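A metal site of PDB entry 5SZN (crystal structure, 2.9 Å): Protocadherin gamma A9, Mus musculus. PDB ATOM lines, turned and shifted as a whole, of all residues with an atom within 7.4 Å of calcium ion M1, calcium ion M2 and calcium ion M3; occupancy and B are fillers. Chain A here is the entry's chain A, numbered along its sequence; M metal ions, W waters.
OD1 of Asn 210 lies close to OE2 of Glu 175 (3.3 Å).
The side-chain carboxylate of Glu 175 lies close to the guanidinium group of Arg 174 (2.8 Å).
OD1 of Asn 210 sits close to OD1 of Asp 209, at 3.1 Å.
OD1 of Asp 295 is in hydrogen-bond range of N of Leu 299, 3.3 Å away.
The side-chain carboxylate (OD1) of Asp 206 sits close to the guanidinium group (NH1) of Arg 174.
The side-chain carboxylate of Asp 206 is in hydrogen-bond range of the backbone NH of Glu 243 (2.7 Å).
NH1 of Arg 174 lies within hydrogen-bond range of O of Pro 241 (3.1 Å).
The side-chain carboxylate (OE1) of Glu 243 is in salt-bridge range of the guanidinium group (NH2) of Arg 174 (3.4 Å).
The nearest printed residue that does not touch calcium ion M1 is Arg 174 (5.3 Å).
Merely in contact with calcium ion M2: Arg 174.
Within 4 Å of calcium ion M2: Glu 116, Arg 174, Glu 175, Asp 206, Thr 207, Asp 209, Asn 210 and Asp 242.
Calcium ion M1 is bound by the side-chain carboxylate of Glu 116 (2.1 Å), the side-chain carboxylate of Asp 173 (2.4 Å), the side-chain carboxylate of Glu 175 (2.5 Å) and the side-chain carboxylate of Asp 209 (2.6 Å).
Calcium ion M1 has four donor atoms within binding distance.
Calcium ion M2 is bound by OE2 of Glu 175 (2.2 Å), OE1 of Glu 116 (2.5 Å), OD1 of Asp 209 (2.7 Å), OD1 of Asp 242 (2.7 Å), O of Thr 207 (2.7 Å), OD1 of Asp 206 (2.8 Å) and OE1 of Glu 175 (3.0 Å).
Calcium ion M2 has seven donor atoms within binding distance.
Calcium ion M3 is bound by OD2 of Asp 242.
Calcium ion M3 is bound by the backbone carbonyl oxygen (O) of Asn 210.
O of Asn 246 is bound to calcium ion M3 (2.4 Å).
OD1 of Asn 208 binds calcium ion M3 (2.5 Å).
Calcium ion M3 is bound by OD2 of Asp 295 (2.6 Å).
OD1 of Asp 240 is bound to calcium ion M3 (2.7 Å).
Calcium ion M3 is bound by OD2 of Asp 240 (2.7 Å).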
ATOM      1  N   GLU A 116      -6.005  29.995   8.698  1.00  0.00           N
ATOM      2  CA  GLU A 116      -4.707  30.499   8.258  1.00  0.00           C
ATOM      3  C   GLU A 116      -4.618  30.529   6.732  1.00  0.00           C
ATOM      4  O   GLU A 116      -3.893  31.357   6.171  1.00  0.00           O
ATOM      5  CB  GLU A 116      -3.596  29.633   8.849  1.00  0.00           C
ATOM      6  CG  GLU A 116      -2.186  30.135   8.601  1.00  0.00           C
ATOM      7  CD  GLU A 116      -1.145  29.196   9.192  1.00  0.00           C
ATOM      8  OE1 GLU A 116      -1.534  28.271   9.936  1.00  0.00           O
ATOM      9  OE2 GLU A 116       0.057  29.387   8.898  1.00  0.00           O
ATOM     10  N   LEU A 172      -3.501  35.892   7.184  1.00  0.00           N
ATOM     11  CA  LEU A 172      -3.183  35.677   8.588  1.00  0.00           C
ATOM     12  C   LEU A 172      -2.188  34.527   8.744  1.00  0.00           C
ATOM     13  O   LEU A 172      -2.010  33.690   7.858  1.00  0.00           O
ATOM     14  CB  LEU A 172      -4.439  35.379   9.394  1.00  0.00           C
ATOM     15  CG  LEU A 172      -5.397  36.572   9.565  1.00  0.00           C
ATOM     16  CD1 LEU A 172      -6.518  36.219  10.521  1.00  0.00           C
ATOM     17  CD2 LEU A 172      -4.631  37.794  10.062  1.00  0.00           C
ATOM     18  N   ASP A 173      -1.518  34.517   9.896  1.00  0.00           N
ATOM     19  CA  ASP A 173      -0.569  33.448  10.229  1.00  0.00           C
ATOM     20  C   ASP A 173      -0.631  33.216  11.724  1.00  0.00           C
ATOM     21  O   ASP A 173      -0.319  34.113  12.514  1.00  0.00           O
ATOM     22  CB  ASP A 173       0.857  33.817   9.803  1.00  0.00           C
ATOM     23  CG  ASP A 173       1.816  32.665   9.936  1.00  0.00           C
ATOM     24  OD1 ASP A 173       1.459  31.533   9.542  1.00  0.00           O
ATOM     25  OD2 ASP A 173       2.940  32.877  10.444  1.00  0.00           O
ATOM     26  N   ARG A 174      -1.045  32.006  12.126  1.00  0.00           N
ATOM     27  CA  ARG A 174      -1.173  31.697  13.537  1.00  0.00           C
ATOM     28  C   ARG A 174       0.187  31.466  14.204  1.00  0.00           C
ATOM     29  O   ARG A 174       0.286  31.602  15.423  1.00  0.00           O
ATOM     30  CB  ARG A 174      -2.039  30.457  13.728  1.00  0.00           C
ATOM     31  CG  ARG A 174      -1.431  29.205  13.153  1.00  0.00           C
ATOM     32  CD  ARG A 174      -2.103  27.955  13.683  1.00  0.00           C
ATOM     33  NE  ARG A 174      -1.972  27.827  15.130  1.00  0.00           N
ATOM     34  CZ  ARG A 174      -0.954  27.230  15.741  1.00  0.00           C
ATOM     35  NH1 ARG A 174       0.041  26.724  15.029  1.00  0.00           N
ATOM     36  NH2 ARG A 174      -0.922  27.161  17.061  1.00  0.00           N
ATOM     37  N   GLU A 175       1.215  31.126  13.422  1.00  0.00           N
ATOM     38  CA  GLU A 175       2.508  30.818  14.006  1.00  0.00           C
ATOM     39  C   GLU A 175       3.170  32.063  14.595  1.00  0.00           C
ATOM     40  O   GLU A 175       3.961  31.962  15.534  1.00  0.00           O
ATOM     41  CB  GLU A 175       3.426  30.185  12.961  1.00  0.00           C
ATOM     42  CG  GLU A 175       3.136  28.715  12.712  1.00  0.00           C
ATOM     43  CD  GLU A 175       1.763  28.470  12.134  1.00  0.00           C
ATOM     44  OE1 GLU A 175       1.331  29.259  11.264  1.00  0.00           O
ATOM     45  OE2 GLU A 175       1.092  27.503  12.551  1.00  0.00           O
ATOM     46  N   GLU A 176       2.842  33.239  14.063  1.00  0.00           N
ATOM     47  CA  GLU A 176       3.370  34.487  14.597  1.00  0.00           C
ATOM     48  C   GLU A 176       2.486  35.044  15.702  1.00  0.00           C
ATOM     49  O   GLU A 176       2.989  35.521  16.729  1.00  0.00           O
ATOM     50  CB  GLU A 176       3.514  35.518  13.476  1.00  0.00           C
ATOM     51  CG  GLU A 176       4.203  34.985  12.226  1.00  0.00           C
ATOM     52  CD  GLU A 176       4.232  35.992  11.090  1.00  0.00           C
ATOM     53  OE1 GLU A 176       4.062  37.198  11.363  1.00  0.00           O
ATOM     54  OE2 GLU A 176       4.418  35.569   9.936  1.00  0.00           O
ATOM     55  N   LEU A 205      -7.383  29.859  12.845  1.00  0.00           N
ATOM     56  CA  LEU A 205      -7.354  28.403  12.805  1.00  0.00           C
ATOM     57  C   LEU A 205      -5.963  27.929  12.377  1.00  0.00           C
ATOM     58  O   LEU A 205      -5.051  28.724  12.118  1.00  0.00           O
ATOM     59  CB  LEU A 205      -8.438  27.863  11.872  1.00  0.00           C
ATOM     60  CG  LEU A 205      -9.880  28.154  12.283  1.00  0.00           C
ATOM     61  CD1 LEU A 205     -10.853  27.408  11.374  1.00  0.00           C
ATOM     62  CD2 LEU A 205     -10.120  27.804  13.742  1.00  0.00           C
ATOM     63  N   ASP A 206      -5.791  26.616  12.296  1.00  0.00           N
ATOM     64  CA  ASP A 206      -4.499  26.018  12.021  1.00  0.00           C
ATOM     65  C   ASP A 206      -4.540  25.284  10.682  1.00  0.00           C
ATOM     66  O   ASP A 206      -5.385  24.409  10.472  1.00  0.00           O
ATOM     67  CB  ASP A 206      -4.074  25.054  13.132  1.00  0.00           C
ATOM     68  CG  ASP A 206      -2.651  24.548  12.955  1.00  0.00           C
ATOM     69  OD1 ASP A 206      -1.893  25.173  12.188  1.00  0.00           O
ATOM     70  OD2 ASP A 206      -2.292  23.541  13.601  1.00  0.00           O
ATOM     71  N   THR A 207      -3.630  25.655   9.789  1.00  0.00           N
ATOM     72  CA  THR A 207      -3.397  24.936   8.545  1.00  0.00           C
ATOM     73  C   THR A 207      -2.037  24.255   8.631  1.00  0.00           C
ATOM     74  O   THR A 207      -1.067  24.842   9.123  1.00  0.00           O
ATOM     75  CB  THR A 207      -3.433  25.886   7.334  1.00  0.00           C
ATOM     76  OG1 THR A 207      -4.720  26.509   7.248  1.00  0.00           O
ATOM     77  CG2 THR A 207      -3.157  25.115   6.044  1.00  0.00           C
ATOM     78  N   ASN A 208      -1.968  23.012   8.166  1.00  0.00           N
ATOM     79  CA  ASN A 208      -0.717  22.262   8.168  1.00  0.00           C
ATOM     80  C   ASN A 208       0.171  22.806   7.041  1.00  0.00           C
ATOM     81  O   ASN A 208       0.306  22.217   5.972  1.00  0.00           O
ATOM     82  CB  ASN A 208      -0.988  20.768   8.008  1.00  0.00           C
ATOM     83  CG  ASN A 208       0.239  19.924   8.277  1.00  0.00           C
ATOM     84  OD1 ASN A 208       1.246  20.413   8.789  1.00  0.00           O
ATOM     85  ND2 ASN A 208       0.154  18.635   7.950  1.00  0.00           N
ATOM     86  N   ASP A 209       0.768  23.958   7.312  1.00  0.00           N
ATOM     87  CA  ASP A 209       1.694  24.597   6.376  1.00  0.00           C
ATOM     88  C   ASP A 209       3.116  24.651   6.926  1.00  0.00           C
ATOM     89  O   ASP A 209       3.989  25.291   6.318  1.00  0.00           O
ATOM     90  CB  ASP A 209       1.204  26.000   6.014  1.00  0.00           C
ATOM     91  CG  ASP A 209       1.050  26.899   7.218  1.00  0.00           C
ATOM     92  OD1 ASP A 209       1.061  26.394   8.349  1.00  0.00           O
ATOM     93  OD2 ASP A 209       0.905  28.124   7.024  1.00  0.00           O
ATOM     94  N   ASN A 210       3.377  24.005   8.067  1.00  0.00           N
ATOM     95  CA  ASN A 210       4.698  23.929   8.659  1.00  0.00           C
ATOM     96  C   ASN A 210       5.205  22.494   8.558  1.00  0.00           C
ATOM     97  O   ASN A 210       4.632  21.583   9.155  1.00  0.00           O
ATOM     98  CB  ASN A 210       4.679  24.378  10.124  1.00  0.00           C
ATOM     99  CG  ASN A 210       4.417  25.854  10.273  1.00  0.00           C
ATOM    100  OD1 ASN A 210       3.277  26.281  10.478  1.00  0.00           O
ATOM    101  ND2 ASN A 210       5.475  26.655  10.178  1.00  0.00           N
ATOM    102  N   ALA A 211       6.295  22.308   7.793  1.00  0.00           N
ATOM    103  CA  ALA A 211       6.918  21.000   7.720  1.00  0.00           C
ATOM    104  C   ALA A 211       7.940  20.829   8.831  1.00  0.00           C
ATOM    105  O   ALA A 211       8.538  21.812   9.289  1.00  0.00           O
ATOM    106  CB  ALA A 211       7.598  20.810   6.364  1.00  0.00           C
ATOM    107  N   PRO A 212       8.155  19.605   9.308  1.00  0.00           N
ATOM    108  CA  PRO A 212       9.165  19.398  10.353  1.00  0.00           C
ATOM    109  C   PRO A 212      10.555  19.751   9.853  1.00  0.00           C
ATOM    110  O   PRO A 212      10.941  19.397   8.735  1.00  0.00           O
ATOM    111  CB  PRO A 212       9.043  17.901  10.664  1.00  0.00           C
ATOM    112  CG  PRO A 212       7.676  17.513  10.199  1.00  0.00           C
ATOM    113  CD  PRO A 212       7.409  18.376   9.002  1.00  0.00           C
ATOM    114  N   SER A 239      11.308  20.338  14.579  1.00  0.00           N
ATOM    115  CA  SER A 239      10.479  21.487  14.921  1.00  0.00           C
ATOM    116  C   SER A 239       9.225  21.487  14.055  1.00  0.00           C
ATOM    117  O   SER A 239       9.316  21.477  12.829  1.00  0.00           O
ATOM    118  CB  SER A 239      11.247  22.795  14.756  1.00  0.00           C
ATOM    119  OG  SER A 239      12.382  22.839  15.592  1.00  0.00           O
ATOM    120  N   ASP A 240       8.064  21.482  14.707  1.00  0.00           N
ATOM    121  CA  ASP A 240       6.781  21.623  14.010  1.00  0.00           C
ATOM    122  C   ASP A 240       5.903  22.562  14.829  1.00  0.00           C
ATOM    123  O   ASP A 240       5.233  22.124  15.790  1.00  0.00           O
ATOM    124  CB  ASP A 240       6.101  20.273  13.812  1.00  0.00           C
ATOM    125  CG  ASP A 240       5.095  20.293  12.668  1.00  0.00           C
ATOM    126  OD1 ASP A 240       4.665  21.395  12.275  1.00  0.00           O
ATOM    127  OD2 ASP A 240       4.745  19.204  12.167  1.00  0.00           O
ATOM    128  N   PRO A 241       5.879  23.852  14.492  1.00  0.00           N
ATOM    129  CA  PRO A 241       5.084  24.811  15.272  1.00  0.00           C
ATOM    130  C   PRO A 241       3.578  24.669  15.093  1.00  0.00           C
ATOM    131  O   PRO A 241       2.834  25.439  15.712  1.00  0.00           O
ATOM    132  CB  PRO A 241       5.560  26.175  14.743  1.00  0.00           C
ATOM    133  CG  PRO A 241       6.846  25.888  14.026  1.00  0.00           C
ATOM    134  CD  PRO A 241       6.694  24.511  13.464  1.00  0.00           C
ATOM    135  N   ASP A 242       3.101  23.716  14.291  1.00  0.00           N
ATOM    136  CA  ASP A 242       1.675  23.536  14.099  1.00  0.00           C
ATOM    137  C   ASP A 242       1.013  23.060  15.388  1.00  0.00           C
ATOM    138  O   ASP A 242       1.654  22.901  16.434  1.00  0.00           O
ATOM    139  CB  ASP A 242       1.414  22.547  12.957  1.00  0.00           C
ATOM    140  CG  ASP A 242       1.712  23.137  11.602  1.00  0.00           C
ATOM    141  OD1 ASP A 242       1.398  24.325  11.383  1.00  0.00           O
ATOM    142  OD2 ASP A 242       2.261  22.415  10.743  1.00  0.00           O
ATOM    143  N   GLU A 243      -0.287  22.821  15.307  1.00  0.00           N
ATOM    144  CA  GLU A 243      -1.100  22.461  16.466  1.00  0.00           C
ATOM    145  C   GLU A 243      -1.777  21.119  16.236  1.00  0.00           C
ATOM    146  O   GLU A 243      -2.286  20.848  15.143  1.00  0.00           O
ATOM    147  CB  GLU A 243      -2.155  23.548  16.747  1.00  0.00           C
ATOM    148  CG  GLU A 243      -2.958  23.317  18.017  1.00  0.00           C
ATOM    149  CD  GLU A 243      -3.855  24.492  18.330  1.00  0.00           C
ATOM    150  OE1 GLU A 243      -3.814  25.496  17.591  1.00  0.00           O
ATOM    151  OE2 GLU A 243      -4.605  24.425  19.331  1.00  0.00           O
ATOM    152  N   ALA A 245      -2.197  17.069  15.714  1.00  0.00           N
ATOM    153  CA  ALA A 245      -1.465  16.050  14.973  1.00  0.00           C
ATOM    154  C   ALA A 245      -0.525  16.664  13.953  1.00  0.00           C
ATOM    155  O   ALA A 245       0.483  16.050  13.585  1.00  0.00           O
ATOM    156  CB  ALA A 245      -2.436  15.089  14.294  1.00  0.00           C
ATOM    157  N   ASN A 246      -0.814  17.888  13.512  1.00  0.00           N
ATOM    158  CA  ASN A 246       0.074  18.577  12.590  1.00  0.00           C
ATOM    159  C   ASN A 246       1.350  19.046  13.263  1.00  0.00           C
ATOM    160  O   ASN A 246       2.259  19.500  12.569  1.00  0.00           O
ATOM    161  CB  ASN A 246      -0.642  19.774  11.963  1.00  0.00           C
ATOM    162  CG  ASN A 246      -1.911  19.371  11.233  1.00  0.00           C
ATOM    163  OD1 ASN A 246      -2.032  18.241  10.749  1.00  0.00           O
ATOM    164  ND2 ASN A 246      -2.849  20.296  11.133  1.00  0.00           N
ATOM    165  N   GLY A 247       1.445  18.958  14.591  1.00  0.00           N
ATOM    166  CA  GLY A 247       2.658  19.347  15.293  1.00  0.00           C
ATOM    167  C   GLY A 247       3.379  18.159  15.898  1.00  0.00           C
ATOM    168  O   GLY A 247       4.428  18.316  16.528  1.00  0.00           O
ATOM    169  N   LYS A 248       2.822  16.964  15.714  1.00  0.00           N
ATOM    170  CA  LYS A 248       3.430  15.735  16.212  1.00  0.00           C
ATOM    171  C   LYS A 248       4.506  15.254  15.256  1.00  0.00           C
ATOM    172  O   LYS A 248       4.464  15.522  14.057  1.00  0.00           O
ATOM    173  CB  LYS A 248       2.356  14.659  16.403  1.00  0.00           C
ATOM    174  CG  LYS A 248       2.843  13.385  17.052  1.00  0.00           C
ATOM    175  CD  LYS A 248       3.441  13.649  18.424  1.00  0.00           C
ATOM    176  CE  LYS A 248       4.186  12.435  18.944  1.00  0.00           C
ATOM    177  NZ  LYS A 248       3.303  11.224  18.962  1.00  0.00           N
ATOM    178  N   GLU A 294       7.964  12.892  10.229  1.00  0.00           N
ATOM    179  CA  GLU A 294       6.688  13.240   9.628  1.00  0.00           C
ATOM    180  C   GLU A 294       5.717  13.701  10.697  1.00  0.00           C
ATOM    181  O   GLU A 294       5.858  13.375  11.880  1.00  0.00           O
ATOM    182  CB  GLU A 294       6.087  12.064   8.848  1.00  0.00           C
ATOM    183  CG  GLU A 294       6.852  11.693   7.590  1.00  0.00           C
ATOM    184  CD  GLU A 294       6.252  10.510   6.861  1.00  0.00           C
ATOM    185  OE1 GLU A 294       5.036  10.261   7.030  1.00  0.00           O
ATOM    186  OE2 GLU A 294       6.990   9.823   6.124  1.00  0.00           O
ATOM    187  N   ASP A 295       4.715  14.462  10.274  1.00  0.00           N
ATOM    188  CA  ASP A 295       3.691  15.008  11.143  1.00  0.00           C
ATOM    189  C   ASP A 295       2.366  14.276  10.899  1.00  0.00           C
ATOM    190  O   ASP A 295       2.373  13.104  10.484  1.00  0.00           O
ATOM    191  CB  ASP A 295       3.618  16.516  10.932  1.00  0.00           C
ATOM    192  CG  ASP A 295       3.310  16.889   9.494  1.00  0.00           C
ATOM    193  OD1 ASP A 295       3.300  15.988   8.631  1.00  0.00           O
ATOM    194  OD2 ASP A 295       3.098  18.097   9.222  1.00  0.00           O
ATOM    195  N   GLY A 296       1.244  14.948  11.164  1.00  0.00           N
ATOM    196  CA  GLY A 296      -0.047  14.336  10.894  1.00  0.00           C
ATOM    197  C   GLY A 296      -0.292  14.127   9.414  1.00  0.00           C
ATOM    198  O   GLY A 296      -0.817  13.079   9.008  1.00  0.00           O
ATOM    199  N   GLY A 297       0.069  15.106   8.590  1.00  0.00           N
ATOM    200  CA  GLY A 297      -0.034  14.985   7.156  1.00  0.00           C
ATOM    201  C   GLY A 297       1.227  14.393   6.539  1.00  0.00           C
ATOM    202  O   GLY A 297       2.097  13.857   7.228  1.00  0.00           O
ATOM    203  N   LEU A 299       3.647  15.860   5.394  1.00  0.00           N
ATOM    204  CA  LEU A 299       4.778  16.768   5.511  1.00  0.00           C
ATOM    205  C   LEU A 299       5.932  16.062   6.225  1.00  0.00           C
ATOM    206  O   LEU A 299       5.735  15.435   7.276  1.00  0.00           O
ATOM    207  CB  LEU A 299       4.369  18.039   6.259  1.00  0.00           C
ATOM    208  CG  LEU A 299       3.559  19.094   5.509  1.00  0.00           C
ATOM    209  CD1 LEU A 299       2.135  18.628   5.256  1.00  0.00           C
ATOM    210  CD2 LEU A 299       3.550  20.409   6.272  1.00  0.00           C
HETATM  211 CA    CA M   1       2.197  29.312   8.960  1.00  0.00          CA
HETATM  212 CA    CA M   2       0.064  26.630  10.833  1.00  0.00          CA
HETATM  213 CA    CA M   3       3.038  20.355  10.459  1.00  0.00          CA
HETATM  214  O   HOH W   1       3.797  29.587   6.037  1.00  0.00           O
